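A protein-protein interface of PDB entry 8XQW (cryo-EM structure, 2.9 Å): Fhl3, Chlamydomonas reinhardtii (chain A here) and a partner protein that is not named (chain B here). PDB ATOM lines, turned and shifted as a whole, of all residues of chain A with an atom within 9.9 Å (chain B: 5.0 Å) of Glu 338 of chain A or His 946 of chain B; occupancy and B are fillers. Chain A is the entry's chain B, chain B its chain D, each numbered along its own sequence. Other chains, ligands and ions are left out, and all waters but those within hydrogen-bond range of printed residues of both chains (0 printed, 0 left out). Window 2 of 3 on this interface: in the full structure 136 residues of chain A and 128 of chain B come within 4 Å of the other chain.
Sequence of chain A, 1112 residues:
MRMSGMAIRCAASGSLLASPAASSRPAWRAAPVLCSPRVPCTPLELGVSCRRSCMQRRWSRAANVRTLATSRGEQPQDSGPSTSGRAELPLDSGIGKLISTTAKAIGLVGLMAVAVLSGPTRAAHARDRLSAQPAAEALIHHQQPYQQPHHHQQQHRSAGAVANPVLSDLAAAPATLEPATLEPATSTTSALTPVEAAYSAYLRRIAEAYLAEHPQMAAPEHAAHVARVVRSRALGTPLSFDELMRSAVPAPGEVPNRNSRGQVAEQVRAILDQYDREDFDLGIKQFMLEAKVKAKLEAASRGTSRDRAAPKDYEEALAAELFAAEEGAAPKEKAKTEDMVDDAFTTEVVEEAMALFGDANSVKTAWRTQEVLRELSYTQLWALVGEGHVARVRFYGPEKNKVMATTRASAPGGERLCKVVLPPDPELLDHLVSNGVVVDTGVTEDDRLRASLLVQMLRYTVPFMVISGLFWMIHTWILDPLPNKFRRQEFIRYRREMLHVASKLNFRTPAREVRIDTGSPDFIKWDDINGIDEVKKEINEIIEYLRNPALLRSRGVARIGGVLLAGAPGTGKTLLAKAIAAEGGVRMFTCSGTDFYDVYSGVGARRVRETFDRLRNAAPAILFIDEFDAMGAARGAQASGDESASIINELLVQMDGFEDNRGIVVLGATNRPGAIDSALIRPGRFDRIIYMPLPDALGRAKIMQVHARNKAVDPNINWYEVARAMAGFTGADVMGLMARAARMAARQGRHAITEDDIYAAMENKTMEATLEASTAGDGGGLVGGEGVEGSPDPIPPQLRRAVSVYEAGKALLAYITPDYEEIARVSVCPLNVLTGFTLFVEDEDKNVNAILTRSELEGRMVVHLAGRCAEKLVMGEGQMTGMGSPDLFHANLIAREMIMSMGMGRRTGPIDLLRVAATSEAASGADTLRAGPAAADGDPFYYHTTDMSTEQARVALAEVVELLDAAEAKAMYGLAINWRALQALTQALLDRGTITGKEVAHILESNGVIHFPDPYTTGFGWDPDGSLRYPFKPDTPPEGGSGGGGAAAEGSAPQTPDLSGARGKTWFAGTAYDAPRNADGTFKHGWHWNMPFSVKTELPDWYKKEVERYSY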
ATOM      1  N   LYS A 334      28.068  11.229  -9.708  1.00  0.00           N
ATOM      2  CA  LYS A 334      26.712  11.055 -10.213  1.00  0.00           C
ATOM      3  C   LYS A 334      26.104   9.768  -9.679  1.00  0.00           C
ATOM      4  O   LYS A 334      26.806   8.916  -9.135  1.00  0.00           O
ATOM      5  CB  LYS A 334      26.698  11.049 -11.744  1.00  0.00           C
ATOM      6  CG  LYS A 334      27.131  12.366 -12.376  1.00  0.00           C
ATOM      7  CD  LYS A 334      26.680  12.473 -13.829  1.00  0.00           C
ATOM      8  CE  LYS A 334      27.179  11.300 -14.664  1.00  0.00           C
ATOM      9  NZ  LYS A 334      26.631  11.316 -16.047  1.00  0.00           N
ATOM     10  N   ALA A 335      24.789   9.637  -9.827  1.00  0.00           N
ATOM     11  CA  ALA A 335      24.098   8.432  -9.390  1.00  0.00           C
ATOM     12  C   ALA A 335      24.089   7.392 -10.501  1.00  0.00           C
ATOM     13  O   ALA A 335      23.917   7.725 -11.675  1.00  0.00           O
ATOM     14  CB  ALA A 335      22.668   8.771  -8.971  1.00  0.00           C
ATOM     15  N   LYS A 336      24.279   6.131 -10.129  1.00  0.00           N
ATOM     16  CA  LYS A 336      24.211   5.042 -11.103  1.00  0.00           C
ATOM     17  C   LYS A 336      23.838   3.717 -10.442  1.00  0.00           C
ATOM     18  O   LYS A 336      23.636   3.653  -9.228  1.00  0.00           O
ATOM     19  CB  LYS A 336      25.528   4.890 -11.884  1.00  0.00           C
ATOM     20  CG  LYS A 336      26.817   4.821 -11.068  1.00  0.00           C
ATOM     21  CD  LYS A 336      27.299   6.190 -10.617  1.00  0.00           C
ATOM     22  CE  LYS A 336      28.594   6.097  -9.829  1.00  0.00           C
ATOM     23  NZ  LYS A 336      28.912   7.394  -9.170  1.00  0.00           N
ATOM     24  N   TPO A 337      23.754   2.671 -11.265  1.00  0.00           N
ATOM     25  CA  TPO A 337      23.169   1.383 -10.887  1.00  0.00           C
ATOM     26  CB  TPO A 337      23.107   0.477 -12.107  1.00  0.00           C
ATOM     27  CG2 TPO A 337      21.785  -0.294 -12.107  1.00  0.00           C
ATOM     28  OG1 TPO A 337      23.159   1.292 -13.276  1.00  0.00           O
ATOM     29  P   TPO A 337      24.572   1.034 -13.995  1.00  0.00           P
ATOM     30  O1P TPO A 337      25.325  -0.189 -13.270  1.00  0.00           O
ATOM     31  O2P TPO A 337      25.463   2.368 -13.893  1.00  0.00           O
ATOM     32  O3P TPO A 337      24.339   0.700 -15.417  1.00  0.00           O
ATOM     33  C   TPO A 337      23.908   0.691  -9.746  1.00  0.00           C
ATOM     34  O   TPO A 337      25.016   1.088  -9.391  1.00  0.00           O
ATOM     35  N   GLU A 338      23.274  -0.333  -9.170  1.00  0.00           N
ATOM     36  CA  GLU A 338      23.696  -0.933  -7.895  1.00  0.00           C
ATOM     37  C   GLU A 338      23.742   0.088  -6.757  1.00  0.00           C
ATOM     38  O   GLU A 338      24.490  -0.060  -5.794  1.00  0.00           O
ATOM     39  CB  GLU A 338      25.049  -1.641  -8.026  1.00  0.00           C
ATOM     40  CG  GLU A 338      25.047  -2.874  -8.923  1.00  0.00           C
ATOM     41  CD  GLU A 338      25.004  -2.559 -10.400  1.00  0.00           C
ATOM     42  OE1 GLU A 338      23.898  -2.319 -10.918  1.00  0.00           O
ATOM     43  OE2 GLU A 338      26.073  -2.568 -11.043  1.00  0.00           O
ATOM     44  N   ASP A 339      22.935   1.134  -6.898  1.00  0.00           N
ATOM     45  CA  ASP A 339      22.633   2.054  -5.816  1.00  0.00           C
ATOM     46  C   ASP A 339      21.153   2.395  -5.781  1.00  0.00           C
ATOM     47  O   ASP A 339      20.705   3.036  -4.825  1.00  0.00           O
ATOM     48  CB  ASP A 339      23.459   3.341  -5.943  1.00  0.00           C
ATOM     49  CG  ASP A 339      24.948   3.071  -6.012  1.00  0.00           C
ATOM     50  OD1 ASP A 339      25.426   2.593  -7.059  1.00  0.00           O
ATOM     51  OD2 ASP A 339      25.644   3.329  -5.010  1.00  0.00           O
ATOM     52  N   MET A 340      20.391   2.005  -6.797  1.00  0.00           N
ATOM     53  CA  MET A 340      18.947   2.147  -6.789  1.00  0.00           C
ATOM     54  C   MET A 340      18.314   1.006  -6.000  1.00  0.00           C
ATOM     55  O   MET A 340      18.809  -0.123  -5.980  1.00  0.00           O
ATOM     56  CB  MET A 340      18.403   2.154  -8.216  1.00  0.00           C
ATOM     57  CG  MET A 340      19.191   3.013  -9.184  1.00  0.00           C
ATOM     58  SD  MET A 340      19.345   4.714  -8.623  1.00  0.00           S
ATOM     59  CE  MET A 340      19.079   5.595 -10.155  1.00  0.00           C
ATOM     60  N   VAL A 341      17.205   1.320  -5.337  1.00  0.00           N
ATOM     61  CA  VAL A 341      16.458   0.315  -4.594  1.00  0.00           C
ATOM     62  C   VAL A 341      15.459  -0.367  -5.526  1.00  0.00           C
ATOM     63  O   VAL A 341      14.917   0.242  -6.451  1.00  0.00           O
ATOM     64  CB  VAL A 341      15.764   0.961  -3.380  1.00  0.00           C
ATOM     65  CG1 VAL A 341      14.980   2.182  -3.820  1.00  0.00           C
ATOM     66  CG2 VAL A 341      14.889  -0.034  -2.642  1.00  0.00           C
ATOM     67  N   ASP A 342      15.207  -1.646  -5.277  1.00  0.00           N
ATOM     68  CA  ASP A 342      14.546  -2.499  -6.268  1.00  0.00           C
ATOM     69  C   ASP A 342      13.044  -2.235  -6.358  1.00  0.00           C
ATOM     70  O   ASP A 342      12.220  -3.127  -6.188  1.00  0.00           O
ATOM     71  CB  ASP A 342      14.825  -3.961  -5.950  1.00  0.00           C
ATOM     72  CG  ASP A 342      16.304  -4.264  -5.878  1.00  0.00           C
ATOM     73  OD1 ASP A 342      17.075  -3.351  -5.521  1.00  0.00           O
ATOM     74  OD2 ASP A 342      16.695  -5.409  -6.185  1.00  0.00           O
ATOM     75  N   ASP A 343      12.689  -0.987  -6.639  1.00  0.00           N
ATOM     76  CA  ASP A 343      11.323  -0.598  -6.972  1.00  0.00           C
ATOM     77  C   ASP A 343      11.364   0.391  -8.130  1.00  0.00           C
ATOM     78  O   ASP A 343      10.718   1.440  -8.117  1.00  0.00           O
ATOM     79  CB  ASP A 343      10.604  -0.023  -5.755  1.00  0.00           C
ATOM     80  CG  ASP A 343       9.964  -1.097  -4.906  1.00  0.00           C
ATOM     81  OD1 ASP A 343       9.334  -2.004  -5.483  1.00  0.00           O
ATOM     82  OD2 ASP A 343      10.088  -1.039  -3.665  1.00  0.00           O
ATOM     83  N   ALA A 344      12.152   0.058  -9.151  1.00  0.00           N
ATOM     84  CA  ALA A 344      12.538   0.998 -10.192  1.00  0.00           C
ATOM     85  C   ALA A 344      11.690   0.886 -11.451  1.00  0.00           C
ATOM     86  O   ALA A 344      12.206   1.089 -12.556  1.00  0.00           O
ATOM     87  CB  ALA A 344      14.016   0.809 -10.530  1.00  0.00           C
ATOM     88  N   SER B 942      15.133 -12.042 -12.123  1.00  0.00           N
ATOM     89  CA  SER B 942      16.353 -11.290 -11.864  1.00  0.00           C
ATOM     90  C   SER B 942      16.816 -10.542 -13.108  1.00  0.00           C
ATOM     91  O   SER B 942      17.328  -9.419 -13.013  1.00  0.00           O
ATOM     92  CB  SER B 942      17.439 -12.234 -11.364  1.00  0.00           C
ATOM     93  OG  SER B 942      17.314 -13.497 -11.990  1.00  0.00           O
ATOM     94  N   THR B 943      16.639 -11.149 -14.285  1.00  0.00           N
ATOM     95  CA  THR B 943      16.999 -10.478 -15.528  1.00  0.00           C
ATOM     96  C   THR B 943      16.238  -9.174 -15.692  1.00  0.00           C
ATOM     97  O   THR B 943      16.845  -8.110 -15.873  1.00  0.00           O
ATOM     98  CB  THR B 943      16.716 -11.397 -16.713  1.00  0.00           C
ATOM     99  OG1 THR B 943      17.397 -12.643 -16.525  1.00  0.00           O
ATOM    100  CG2 THR B 943      17.181 -10.755 -18.005  1.00  0.00           C
ATOM    101  N   ARG B 944      14.906  -9.245 -15.638  1.00  0.00           N
ATOM    102  CA  ARG B 944      14.088  -8.048 -15.770  1.00  0.00           C
ATOM    103  C   ARG B 944      14.381  -7.054 -14.658  1.00  0.00           C
ATOM    104  O   ARG B 944      14.347  -5.840 -14.883  1.00  0.00           O
ATOM    105  CB  ARG B 944      12.610  -8.433 -15.772  1.00  0.00           C
ATOM    106  CG  ARG B 944      12.142  -9.049 -17.073  1.00  0.00           C
ATOM    107  CD  ARG B 944      11.185 -10.193 -16.823  1.00  0.00           C
ATOM    108  NE  ARG B 944      10.493 -10.594 -18.042  1.00  0.00           N
ATOM    109  CZ  ARG B 944       9.629 -11.599 -18.107  1.00  0.00           C
ATOM    110  NH1 ARG B 944       9.355 -12.304 -17.019  1.00  0.00           N
ATOM    111  NH2 ARG B 944       9.039 -11.899 -19.256  1.00  0.00           N
ATOM    112  N   LEU B 945      14.675  -7.547 -13.453  1.00  0.00           N
ATOM    113  CA  LEU B 945      14.990  -6.649 -12.348  1.00  0.00           C
ATOM    114  C   LEU B 945      16.231  -5.825 -12.650  1.00  0.00           C
ATOM    115  O   LEU B 945      16.233  -4.597 -12.473  1.00  0.00           O
ATOM    116  CB  LEU B 945      15.175  -7.451 -11.063  1.00  0.00           C
ATOM    117  CG  LEU B 945      15.805  -6.741  -9.863  1.00  0.00           C
ATOM    118  CD1 LEU B 945      14.992  -5.527  -9.448  1.00  0.00           C
ATOM    119  CD2 LEU B 945      15.959  -7.707  -8.699  1.00  0.00           C
ATOM    120  N   HIS B 946      17.297  -6.479 -13.111  1.00  0.00           N
ATOM    121  CA  HIS B 946      18.514  -5.739 -13.413  1.00  0.00           C
ATOM    122  C   HIS B 946      18.314  -4.830 -14.618  1.00  0.00           C
ATOM    123  O   HIS B 946      18.866  -3.726 -14.667  1.00  0.00           O
ATOM    124  CB  HIS B 946      19.676  -6.701 -13.632  1.00  0.00           C
ATOM    125  CG  HIS B 946      20.993  -6.148 -13.190  1.00  0.00           C
ATOM    126  ND1 HIS B 946      22.185  -6.814 -13.377  1.00  0.00           N
ATOM    127  CD2 HIS B 946      21.304  -4.986 -12.572  1.00  0.00           C
ATOM    128  CE1 HIS B 946      23.174  -6.086 -12.892  1.00  0.00           C
ATOM    129  NE2 HIS B 946      22.667  -4.970 -12.399  1.00  0.00           N
ATOM    130  N   ILE B 947      17.511  -5.269 -15.589  1.00  0.00           N
ATOM    131  CA  ILE B 947      17.168  -4.409 -16.716  1.00  0.00           C
ATOM    132  C   ILE B 947      16.517  -3.121 -16.227  1.00  0.00           C
ATOM    133  O   ILE B 947      16.880  -2.016 -16.653  1.00  0.00           O
ATOM    134  CB  ILE B 947      16.243  -5.161 -17.687  1.00  0.00           C
ATOM    135  CG1 ILE B 947      17.033  -6.167 -18.516  1.00  0.00           C
ATOM    136  CG2 ILE B 947      15.509  -4.190 -18.578  1.00  0.00           C
ATOM    137  CD1 ILE B 947      16.173  -7.278 -19.061  1.00  0.00           C
ATOM    138  N   GLN B 948      15.535  -3.248 -15.336  1.00  0.00           N
ATOM    139  CA  GLN B 948      14.812  -2.083 -14.844  1.00  0.00           C
ATOM    140  C   GLN B 948      15.736  -1.168 -14.056  1.00  0.00           C
ATOM    141  O   GLN B 948      15.678   0.062 -14.185  1.00  0.00           O
ATOM    142  CB  GLN B 948      13.636  -2.535 -13.980  1.00  0.00           C
ATOM    143  CG  GLN B 948      12.277  -2.080 -14.477  1.00  0.00           C
ATOM    144  CD  GLN B 948      11.164  -2.440 -13.518  1.00  0.00           C
ATOM    145  OE1 GLN B 948      11.379  -2.531 -12.310  1.00  0.00           O
ATOM    146  NE2 GLN B 948       9.966  -2.638 -14.048  1.00  0.00           N
ATOM    147  N   LYS B 949      16.601  -1.756 -13.226  1.00  0.00           N
ATOM    148  CA  LYS B 949      17.542  -0.936 -12.474  1.00  0.00           C
ATOM    149  C   LYS B 949      18.473  -0.176 -13.408  1.00  0.00           C
ATOM    150  O   LYS B 949      18.759   1.005 -13.183  1.00  0.00           O
ATOM    151  CB  LYS B 949      18.335  -1.802 -11.496  1.00  0.00           C
ATOM    152  CG  LYS B 949      17.469  -2.494 -10.458  1.00  0.00           C
ATOM    153  CD  LYS B 949      18.160  -3.698  -9.862  1.00  0.00           C
ATOM    154  CE  LYS B 949      19.260  -3.260  -8.929  1.00  0.00           C
ATOM    155  NZ  LYS B 949      18.887  -2.001  -8.238  1.00  0.00           N
ATOM    156  N   LYS B 950      18.923  -0.826 -14.483  1.00  0.00           N
ATOM    157  CA  LYS B 950      19.809  -0.163 -15.434  1.00  0.00           C
ATOM    158  C   LYS B 950      19.098   0.981 -16.144  1.00  0.00           C
ATOM    159  O   LYS B 950      19.654   2.076 -16.290  1.00  0.00           O
ATOM    160  CB  LYS B 950      20.341  -1.175 -16.448  1.00  0.00           C
ATOM    161  CG  LYS B 950      21.583  -0.707 -17.186  1.00  0.00           C
ATOM    162  CD  LYS B 950      22.509  -1.867 -17.496  1.00  0.00           C
ATOM    163  CE  LYS B 950      22.897  -2.618 -16.233  1.00  0.00           C
ATOM    164  NZ  LYS B 950      23.253  -1.710 -15.109  1.00  0.00           N
ATOM    165  N   ARG B 951      17.866   0.746 -16.593  1.00  0.00           N
ATOM    166  CA  ARG B 951      17.139   1.791 -17.301  1.00  0.00           C
ATOM    167  C   ARG B 951      16.864   2.984 -16.398  1.00  0.00           C
ATOM    168  O   ARG B 951      16.944   4.140 -16.837  1.00  0.00           O
ATOM    169  CB  ARG B 951      15.835   1.237 -17.868  1.00  0.00           C
ATOM    170  CG  ARG B 951      15.453   1.814 -19.217  1.00  0.00           C
ATOM    171  CD  ARG B 951      14.834   3.188 -19.068  1.00  0.00           C
ATOM    172  NE  ARG B 951      14.138   3.615 -20.276  1.00  0.00           N
ATOM    173  CZ  ARG B 951      14.652   4.442 -21.179  1.00  0.00           C
ATOM    174  NH1 ARG B 951      15.871   4.934 -21.011  1.00  0.00           N
ATOM    175  NH2 ARG B 951      13.949   4.780 -22.250  1.00  0.00           N
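Hydrophobic or aromatic side chains of chain B within 4 Å of the printed part of chain A: Leu 945 and His 946.
Among the printed residues, Asp or Glu carboxylates within 4 Å of a Lys or Arg side-chain nitrogen of the other chain: Asp 342 of chain A with Lys 949 of chain B.
Among the printed residues, pairs that only touch across the chains: TPO 337 of chain A with Lys 949 of chain B (3.5 Å), Asp 342 of chain A with Leu 945 of chain B (3.5 Å) and Ala 344 of chain A with Gln 948 of chain B (3.5 Å).
The backbone carbonyl oxygen (O) of Met 340 of chain A is in hydrogen-bond range of the side-chain amino group (NZ) of Lys 949 of chain B, at 2.9 Å.
The side-chain carboxylate (OE1) of Glu 338 of chain A lies within hydrogen-bond range of a ring nitrogen (NE2) of His 946 of chain B.
O3P of TPO 337 of chain A sits close to the side-chain amino group (NZ) of Lys 950 of chain B (2.7 Å).
OD1 of Asp 342 of chain A is in salt-bridge range of NZ of Lys 949 of chain B (3.5 Å).
Lys 334 of chain A touches none of the printed residues of chain B.
Printed residues of chain B within 4 Å of TPO 337 of chain A: Lys 949 (3.5 Å) and Lys 950 (2.7 Å).
Of the printed residues of chain B, Asp 342 of chain A touches Leu 945 (3.5 Å) and Lys 949 (3.5 Å).
Printed residues of chain B within 4 Å of Ala 344 of chain A: Gln 948.
Arg 944 of chain B touches none of the printed residues of chain A.
Leu 945 of chain B touches one residue of chain A.
His 946 of chain B touches just one residue of chain A: Glu 338.
No residue of chain A comes within 4 Å of Ile 947 of chain B.
Of the printed residues of chain A, Gln 948 of chain B touches Ala 344 (3.5 Å).
Lys 949 of chain B touches just these residues of chain A: TPO 337, Met 340 and Asp 342.
Of the printed residues of chain A, Lys 950 of chain B touches TPO 337.
The nearest residue of chain A that does not touch His 946 of chain B is TPO 337 of chain A (4.7 Å).
The nearest printed residue of chain B that does not touch Ala 344 of chain A is Lys 949 of chain B (4.4 Å).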
